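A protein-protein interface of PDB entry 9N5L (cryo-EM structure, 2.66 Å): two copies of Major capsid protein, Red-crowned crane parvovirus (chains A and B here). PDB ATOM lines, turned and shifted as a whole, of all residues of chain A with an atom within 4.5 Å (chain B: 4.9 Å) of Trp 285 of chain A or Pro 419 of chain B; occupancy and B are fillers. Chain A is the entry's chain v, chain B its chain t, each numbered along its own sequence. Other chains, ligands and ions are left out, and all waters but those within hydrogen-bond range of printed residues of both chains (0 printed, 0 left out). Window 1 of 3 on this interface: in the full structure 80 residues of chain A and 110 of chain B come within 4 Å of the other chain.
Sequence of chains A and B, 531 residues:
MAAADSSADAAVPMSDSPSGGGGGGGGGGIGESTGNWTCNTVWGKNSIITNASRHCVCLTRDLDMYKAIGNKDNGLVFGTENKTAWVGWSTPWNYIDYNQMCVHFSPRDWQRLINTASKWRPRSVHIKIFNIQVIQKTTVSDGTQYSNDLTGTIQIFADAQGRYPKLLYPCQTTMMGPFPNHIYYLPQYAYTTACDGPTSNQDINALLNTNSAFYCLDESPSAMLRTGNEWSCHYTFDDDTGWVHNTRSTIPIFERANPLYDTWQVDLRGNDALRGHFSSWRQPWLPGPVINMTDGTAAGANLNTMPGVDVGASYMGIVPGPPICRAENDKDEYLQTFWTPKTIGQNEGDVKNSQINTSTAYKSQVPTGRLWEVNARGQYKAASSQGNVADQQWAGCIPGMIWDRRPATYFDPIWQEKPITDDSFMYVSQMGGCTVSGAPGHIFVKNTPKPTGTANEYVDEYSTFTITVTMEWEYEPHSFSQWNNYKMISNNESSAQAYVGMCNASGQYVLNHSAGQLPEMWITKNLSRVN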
ATOM      1  N   ILE A 253      24.917  33.754 -25.657  1.00  0.00           N
ATOM      2  CA  ILE A 253      23.942  32.764 -25.214  1.00  0.00           C
ATOM      3  C   ILE A 253      22.557  33.107 -25.741  1.00  0.00           C
ATOM      4  O   ILE A 253      21.682  32.242 -25.838  1.00  0.00           O
ATOM      5  CB  ILE A 253      23.947  32.645 -23.681  1.00  0.00           C
ATOM      6  CG1 ILE A 253      23.510  33.959 -23.042  1.00  0.00           C
ATOM      7  CG2 ILE A 253      25.320  32.258 -23.190  1.00  0.00           C
ATOM      8  CD1 ILE A 253      23.246  33.840 -21.578  1.00  0.00           C
ATOM      9  N   ARG A 256      21.903  31.593 -30.060  1.00  0.00           N
ATOM     10  CA  ARG A 256      22.335  30.219 -30.178  1.00  0.00           C
ATOM     11  C   ARG A 256      21.724  29.534 -31.387  1.00  0.00           C
ATOM     12  O   ARG A 256      22.028  28.375 -31.665  1.00  0.00           O
ATOM     13  CB  ARG A 256      22.023  29.500 -28.874  1.00  0.00           C
ATOM     14  CG  ARG A 256      22.543  28.125 -28.788  1.00  0.00           C
ATOM     15  CD  ARG A 256      24.044  28.030 -28.950  1.00  0.00           C
ATOM     16  NE  ARG A 256      24.797  28.709 -27.910  1.00  0.00           N
ATOM     17  CZ  ARG A 256      26.104  28.557 -27.754  1.00  0.00           C
ATOM     18  NH1 ARG A 256      26.758  27.714 -28.535  1.00  0.00           N
ATOM     19  NH2 ARG A 256      26.744  29.199 -26.789  1.00  0.00           N
ATOM     20  N   GLN A 283      14.063  32.254 -25.001  1.00  0.00           N
ATOM     21  CA  GLN A 283      15.236  31.426 -24.827  1.00  0.00           C
ATOM     22  C   GLN A 283      15.014  30.277 -23.879  1.00  0.00           C
ATOM     23  O   GLN A 283      14.231  30.370 -22.944  1.00  0.00           O
ATOM     24  CB  GLN A 283      16.395  32.285 -24.332  1.00  0.00           C
ATOM     25  CG  GLN A 283      16.583  33.573 -25.113  1.00  0.00           C
ATOM     26  CD  GLN A 283      17.253  33.349 -26.449  1.00  0.00           C
ATOM     27  OE1 GLN A 283      18.010  32.402 -26.619  1.00  0.00           O
ATOM     28  NE2 GLN A 283      16.978  34.222 -27.403  1.00  0.00           N
ATOM     29  N   PRO A 284      15.690  29.163 -24.168  1.00  0.00           N
ATOM     30  CA  PRO A 284      15.659  27.900 -23.429  1.00  0.00           C
ATOM     31  C   PRO A 284      16.464  27.993 -22.148  1.00  0.00           C
ATOM     32  O   PRO A 284      16.556  27.033 -21.394  1.00  0.00           O
ATOM     33  CB  PRO A 284      16.335  26.913 -24.387  1.00  0.00           C
ATOM     34  CG  PRO A 284      16.736  27.690 -25.598  1.00  0.00           C
ATOM     35  CD  PRO A 284      16.679  29.137 -25.250  1.00  0.00           C
ATOM     36  N   TRP A 285      17.059  29.151 -21.924  1.00  0.00           N
ATOM     37  CA  TRP A 285      17.866  29.388 -20.758  1.00  0.00           C
ATOM     38  C   TRP A 285      17.919  30.870 -20.506  1.00  0.00           C
ATOM     39  O   TRP A 285      17.533  31.678 -21.340  1.00  0.00           O
ATOM     40  CB  TRP A 285      19.282  28.888 -20.998  1.00  0.00           C
ATOM     41  CG  TRP A 285      19.785  29.300 -22.326  1.00  0.00           C
ATOM     42  CD1 TRP A 285      20.140  30.553 -22.713  1.00  0.00           C
ATOM     43  CD2 TRP A 285      19.961  28.461 -23.463  1.00  0.00           C
ATOM     44  NE1 TRP A 285      20.536  30.546 -24.020  1.00  0.00           N
ATOM     45  CE2 TRP A 285      20.437  29.271 -24.504  1.00  0.00           C
ATOM     46  CE3 TRP A 285      19.770  27.103 -23.701  1.00  0.00           C
ATOM     47  CZ2 TRP A 285      20.723  28.767 -25.761  1.00  0.00           C
ATOM     48  CZ3 TRP A 285      20.052  26.606 -24.945  1.00  0.00           C
ATOM     49  CH2 TRP A 285      20.524  27.433 -25.963  1.00  0.00           C
ATOM     50  N   LEU A 286      18.369  31.211 -19.317  1.00  0.00           N
ATOM     51  CA  LEU A 286      18.554  32.590 -18.928  1.00  0.00           C
ATOM     52  C   LEU A 286      19.913  32.683 -18.258  1.00  0.00           C
ATOM     53  O   LEU A 286      20.468  31.686 -17.804  1.00  0.00           O
ATOM     54  CB  LEU A 286      17.442  33.080 -18.005  1.00  0.00           C
ATOM     55  CG  LEU A 286      17.030  32.211 -16.823  1.00  0.00           C
ATOM     56  CD1 LEU A 286      16.306  33.070 -15.805  1.00  0.00           C
ATOM     57  CD2 LEU A 286      16.133  31.083 -17.296  1.00  0.00           C
ATOM     58  N   GLY A 400      16.966  27.202 -14.792  1.00  0.00           N
ATOM     59  CA  GLY A 400      17.301  27.504 -16.169  1.00  0.00           C
ATOM     60  C   GLY A 400      18.276  28.651 -16.328  1.00  0.00           C
ATOM     61  O   GLY A 400      18.544  29.087 -17.438  1.00  0.00           O
ATOM     62  N   ILE A 402      21.876  30.277 -16.441  1.00  0.00           N
ATOM     63  CA  ILE A 402      23.246  29.887 -16.747  1.00  0.00           C
ATOM     64  C   ILE A 402      24.112  31.134 -16.743  1.00  0.00           C
ATOM     65  O   ILE A 402      23.726  32.159 -17.285  1.00  0.00           O
ATOM     66  CB  ILE A 402      23.361  29.181 -18.105  1.00  0.00           C
ATOM     67  CG1 ILE A 402      22.979  30.130 -19.237  1.00  0.00           C
ATOM     68  CG2 ILE A 402      22.498  27.934 -18.129  1.00  0.00           C
ATOM     69  CD1 ILE A 402      23.205  29.546 -20.610  1.00  0.00           C
ATOM     70  N   ASN A 531      31.285  26.120 -27.437  1.00  0.00           N
ATOM     71  CA  ASN A 531      29.859  26.106 -27.177  1.00  0.00           C
ATOM     72  C   ASN A 531      29.495  26.643 -25.802  1.00  0.00           C
ATOM     73  O   ASN A 531      28.393  26.408 -25.313  1.00  0.00           O
ATOM     74  CB  ASN A 531      29.326  24.688 -27.350  1.00  0.00           C
ATOM     75  CG  ASN A 531      29.392  24.228 -28.783  1.00  0.00           C
ATOM     76  OD1 ASN A 531      28.612  24.665 -29.619  1.00  0.00           O
ATOM     77  ND2 ASN A 531      30.325  23.340 -29.074  1.00  0.00           N
ATOM     78  OXT ASN A 531      30.279  27.329 -25.153  1.00  0.00           O
ATOM     79  N   LEU B 168      21.747  25.228 -30.593  1.00  0.00           N
ATOM     80  CA  LEU B 168      21.028  24.664 -29.465  1.00  0.00           C
ATOM     81  C   LEU B 168      19.606  25.177 -29.407  1.00  0.00           C
ATOM     82  O   LEU B 168      18.827  24.761 -28.547  1.00  0.00           O
ATOM     83  CB  LEU B 168      21.759  24.987 -28.172  1.00  0.00           C
ATOM     84  CG  LEU B 168      23.203  24.532 -28.135  1.00  0.00           C
ATOM     85  CD1 LEU B 168      23.851  25.023 -26.876  1.00  0.00           C
ATOM     86  CD2 LEU B 168      23.255  23.039 -28.226  1.00  0.00           C
ATOM     87  N   TYR B 169      19.251  26.084 -30.291  1.00  0.00           N
ATOM     88  CA  TYR B 169      17.967  26.732 -30.153  1.00  0.00           C
ATOM     89  C   TYR B 169      16.885  25.772 -30.623  1.00  0.00           C
ATOM     90  O   TYR B 169      16.998  25.203 -31.716  1.00  0.00           O
ATOM     91  CB  TYR B 169      17.916  28.024 -30.949  1.00  0.00           C
ATOM     92  CG  TYR B 169      16.701  28.830 -30.630  1.00  0.00           C
ATOM     93  CD1 TYR B 169      16.668  29.622 -29.500  1.00  0.00           C
ATOM     94  CD2 TYR B 169      15.578  28.775 -31.426  1.00  0.00           C
ATOM     95  CE1 TYR B 169      15.566  30.356 -29.187  1.00  0.00           C
ATOM     96  CE2 TYR B 169      14.468  29.506 -31.116  1.00  0.00           C
ATOM     97  CZ  TYR B 169      14.467  30.296 -29.996  1.00  0.00           C
ATOM     98  OH  TYR B 169      13.352  31.031 -29.687  1.00  0.00           O
ATOM     99  N   MET B 316      18.202  40.011 -23.553  1.00  0.00           N
ATOM    100  CA  MET B 316      17.746  38.629 -23.490  1.00  0.00           C
ATOM    101  C   MET B 316      16.521  38.594 -22.587  1.00  0.00           C
ATOM    102  O   MET B 316      16.577  39.063 -21.460  1.00  0.00           O
ATOM    103  CB  MET B 316      18.833  37.716 -22.947  1.00  0.00           C
ATOM    104  CG  MET B 316      18.500  36.243 -23.059  1.00  0.00           C
ATOM    105  SD  MET B 316      19.882  35.197 -22.588  1.00  0.00           S
ATOM    106  CE  MET B 316      19.227  33.569 -22.924  1.00  0.00           C
ATOM    107  N   GLN B 416      17.261  19.560 -24.693  1.00  0.00           N
ATOM    108  CA  GLN B 416      17.682  20.933 -24.825  1.00  0.00           C
ATOM    109  C   GLN B 416      19.083  20.998 -24.273  1.00  0.00           C
ATOM    110  O   GLN B 416      19.328  20.602 -23.143  1.00  0.00           O
ATOM    111  CB  GLN B 416      16.776  21.876 -24.054  1.00  0.00           C
ATOM    112  CG  GLN B 416      17.260  23.310 -24.101  1.00  0.00           C
ATOM    113  CD  GLN B 416      17.496  23.790 -25.513  1.00  0.00           C
ATOM    114  OE1 GLN B 416      16.595  23.770 -26.338  1.00  0.00           O
ATOM    115  NE2 GLN B 416      18.709  24.227 -25.795  1.00  0.00           N
ATOM    116  N   GLU B 417      20.008  21.511 -25.065  1.00  0.00           N
ATOM    117  CA  GLU B 417      21.372  21.616 -24.609  1.00  0.00           C
ATOM    118  C   GLU B 417      21.634  23.073 -24.322  1.00  0.00           C
ATOM    119  O   GLU B 417      21.486  23.916 -25.193  1.00  0.00           O
ATOM    120  CB  GLU B 417      22.318  21.110 -25.686  1.00  0.00           C
ATOM    121  CG  GLU B 417      23.734  20.873 -25.213  1.00  0.00           C
ATOM    122  CD  GLU B 417      24.492  19.937 -26.126  1.00  0.00           C
ATOM    123  OE1 GLU B 417      23.962  19.607 -27.206  1.00  0.00           O
ATOM    124  OE2 GLU B 417      25.612  19.525 -25.761  1.00  0.00           O
ATOM    125  N   LYS B 418      21.978  23.373 -23.079  1.00  0.00           N
ATOM    126  CA  LYS B 418      22.276  24.736 -22.689  1.00  0.00           C
ATOM    127  C   LYS B 418      23.672  25.083 -23.155  1.00  0.00           C
ATOM    128  O   LYS B 418      24.503  24.199 -23.326  1.00  0.00           O
ATOM    129  CB  LYS B 418      22.172  24.898 -21.176  1.00  0.00           C
ATOM    130  CG  LYS B 418      22.901  23.816 -20.409  1.00  0.00           C
ATOM    131  CD  LYS B 418      22.950  24.120 -18.928  1.00  0.00           C
ATOM    132  CE  LYS B 418      23.703  23.033 -18.193  1.00  0.00           C
ATOM    133  NZ  LYS B 418      23.960  23.411 -16.780  1.00  0.00           N
ATOM    134  N   PRO B 419      23.938  26.374 -23.370  1.00  0.00           N
ATOM    135  CA  PRO B 419      25.275  26.805 -23.771  1.00  0.00           C
ATOM    136  C   PRO B 419      26.242  26.534 -22.633  1.00  0.00           C
ATOM    137  O   PRO B 419      25.884  26.700 -21.472  1.00  0.00           O
ATOM    138  CB  PRO B 419      25.112  28.313 -23.964  1.00  0.00           C
ATOM    139  CG  PRO B 419      23.658  28.518 -24.185  1.00  0.00           C
ATOM    140  CD  PRO B 419      22.990  27.494 -23.327  1.00  0.00           C
ATOM    141  N   ILE B 420      27.460  26.125 -22.950  1.00  0.00           N
ATOM    142  CA  ILE B 420      28.419  25.843 -21.902  1.00  0.00           C
ATOM    143  C   ILE B 420      28.726  27.099 -21.108  1.00  0.00           C
ATOM    144  O   ILE B 420      28.935  28.170 -21.668  1.00  0.00           O
ATOM    145  CB  ILE B 420      29.729  25.294 -22.476  1.00  0.00           C
ATOM    146  CG1 ILE B 420      29.487  23.941 -23.137  1.00  0.00           C
ATOM    147  CG2 ILE B 420      30.777  25.181 -21.383  1.00  0.00           C
ATOM    148  CD1 ILE B 420      30.708  23.373 -23.815  1.00  0.00           C
ATOM    149  N   THR B 421      28.753  26.946 -19.794  1.00  0.00           N
ATOM    150  CA  THR B 421      29.044  28.036 -18.884  1.00  0.00           C
ATOM    151  C   THR B 421      29.688  27.435 -17.654  1.00  0.00           C
ATOM    152  O   THR B 421      29.681  26.219 -17.462  1.00  0.00           O
ATOM    153  CB  THR B 421      27.790  28.822 -18.490  1.00  0.00           C
ATOM    154  OG1 THR B 421      26.828  27.927 -17.925  1.00  0.00           O
ATOM    155  CG2 THR B 421      27.184  29.522 -19.678  1.00  0.00           C
ATOM    156  N   TYR B 427      19.029  23.598 -14.366  1.00  0.00           N
ATOM    157  CA  TYR B 427      18.671  23.993 -15.715  1.00  0.00           C
ATOM    158  C   TYR B 427      17.442  23.248 -16.206  1.00  0.00           C
ATOM    159  O   TYR B 427      17.380  22.019 -16.159  1.00  0.00           O
ATOM    160  CB  TYR B 427      19.824  23.765 -16.680  1.00  0.00           C
ATOM    161  CG  TYR B 427      19.379  24.056 -18.076  1.00  0.00           C
ATOM    162  CD1 TYR B 427      19.108  25.350 -18.463  1.00  0.00           C
ATOM    163  CD2 TYR B 427      19.211  23.046 -19.003  1.00  0.00           C
ATOM    164  CE1 TYR B 427      18.683  25.634 -19.716  1.00  0.00           C
ATOM    165  CE2 TYR B 427      18.787  23.323 -20.271  1.00  0.00           C
ATOM    166  CZ  TYR B 427      18.525  24.624 -20.620  1.00  0.00           C
ATOM    167  OH  TYR B 427      18.104  24.937 -21.880  1.00  0.00           O
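The backbone carbonyl oxygen (O) of Arg 256 of chain A is in hydrogen-bond range of the backbone NH (N) of Leu 168 of chain B (3.3 Å).
N of Ile 420 of chain B is in hydrogen-bond range of O of Asn 531 of chain A (2.6 Å).
The side-chain hydroxyl (OH) of Tyr 427 of chain B sits at hydrogen-bond distance from the backbone carbonyl oxygen (O) of Pro 284 of chain A (2.7 Å).
The backbone carbonyl oxygen of Leu 168 of chain B is in hydrogen-bond range of the side-chain amide nitrogen of Gln 416 of chain B (2.8 Å).
The backbone carbonyl oxygen (O) of Ile 253 of chain A sits at hydrogen-bond distance from the indole nitrogen (NE1) of Trp 285 of chain A, 2.7 Å away.
The guanidinium group (NH2) of Arg 256 of chain A is in salt-bridge range of the chain-end carboxylate (O) of Asn 531 of chain A (3.6 Å).
O of Gly 400 of chain A is in hydrogen-bond range of N of Leu 286 of chain A (2.8 Å).
The backbone carbonyl oxygen (O) of Leu 286 of chain A lies within hydrogen-bond range of the backbone NH (N) of Ile 402 of chain A (2.4 Å).
Among the printed residues, merely in contact across the chains: Ile 253 of chain A with Met 316 of chain B (3.8 Å), Arg 256 of chain A with Tyr 169 of chain B (3.9 Å), Arg 256 of chain A with Pro 419 of chain B (3.4 Å), Gln 283 of chain A with Met 316 of chain B (3.4 Å), Pro 284 of chain A with Gln 416 of chain B (3.5 Å), Trp 285 of chain A with Leu 168 of chain B (3.5 Å), Trp 285 of chain A with Met 316 of chain B (3.0 Å), Trp 285 of chain A with Gln 416 of chain B (2.9 Å), Trp 285 of chain A with Glu 417 of chain B (3.1 Å), Trp 285 of chain A with Lys 418 of chain B (3.6 Å), Trp 285 of chain A with Pro 419 of chain B (3.2 Å), Trp 285 of chain A with Tyr 427 of chain B (3.3 Å), Gly 400 of chain A with Tyr 427 of chain B (3.6 Å), Ile 402 of chain A with Lys 418 of chain B (3.9 Å), Ile 402 of chain A with Pro 419 of chain B (3.4 Å), Ile 402 of chain A with Thr 421 of chain B (3.7 Å) and Asn 531 of chain A with Pro 419 of chain B (3.4 Å).
Of the printed residues of chain B, Ile 253 of chain A touches Met 316 (3.8 Å).
Printed residues of chain B within 4 Å of Pro 284 of chain A: Gln 416 and Tyr 427.
Trp 285 of chain A touches seven residues of chain B.
Leu 286 of chain A touches none of the printed residues of chain B.
Printed residues of chain B within 4 Å of Ile 402 of chain A: Lys 418 (3.9 Å), Pro 419 (3.4 Å) and Thr 421 (3.7 Å).
Printed residues of chain A within 4 Å of Leu 168 of chain B: Arg 256 (3.3 Å) and Trp 285 (3.5 Å).
Of chain A, only Arg 256, Trp 285, Ile 402 and Asn 531 come within 4 Å of Pro 419 of chain B.
Of the printed residues of chain A, Thr 421 of chain B touches Ile 402.
The nearest residue of chain A that does not touch Pro 419 of chain B is Ile 253 of chain A (4.03 Å).
Of the 10 printed residues of chain B, 10 touch a printed residue of chain A.
Printed residues of chain B that touch a printed residue of chain A: Leu 168, Tyr 169, Met 316, Gln 416, Glu 417, Lys 418, Pro 419, Ile 420, Thr 421 and Tyr 427.
Of the 9 printed residues of chain A, 8 touch a printed residue of chain B.
Printed residues of chain A that touch a printed residue of chain B: Ile 253, Arg 256, Gln 283, Pro 284, Trp 285, Gly 400, Ile 402 and Asn 531.
Hydrophobic or aromatic side chains of chain A that line the printed part of chain B: Ile 253, Pro 284, Trp 285 and Ile 402.
Among the printed residues, no Asp or Glu carboxylate lies within 4 Å of a Lys or Arg side-chain nitrogen of the other chain.
No position is printed for both chains.
Of the 20 pairs that touch across the chains among the printed residues, none has its exchanged pair printed and touching as well.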
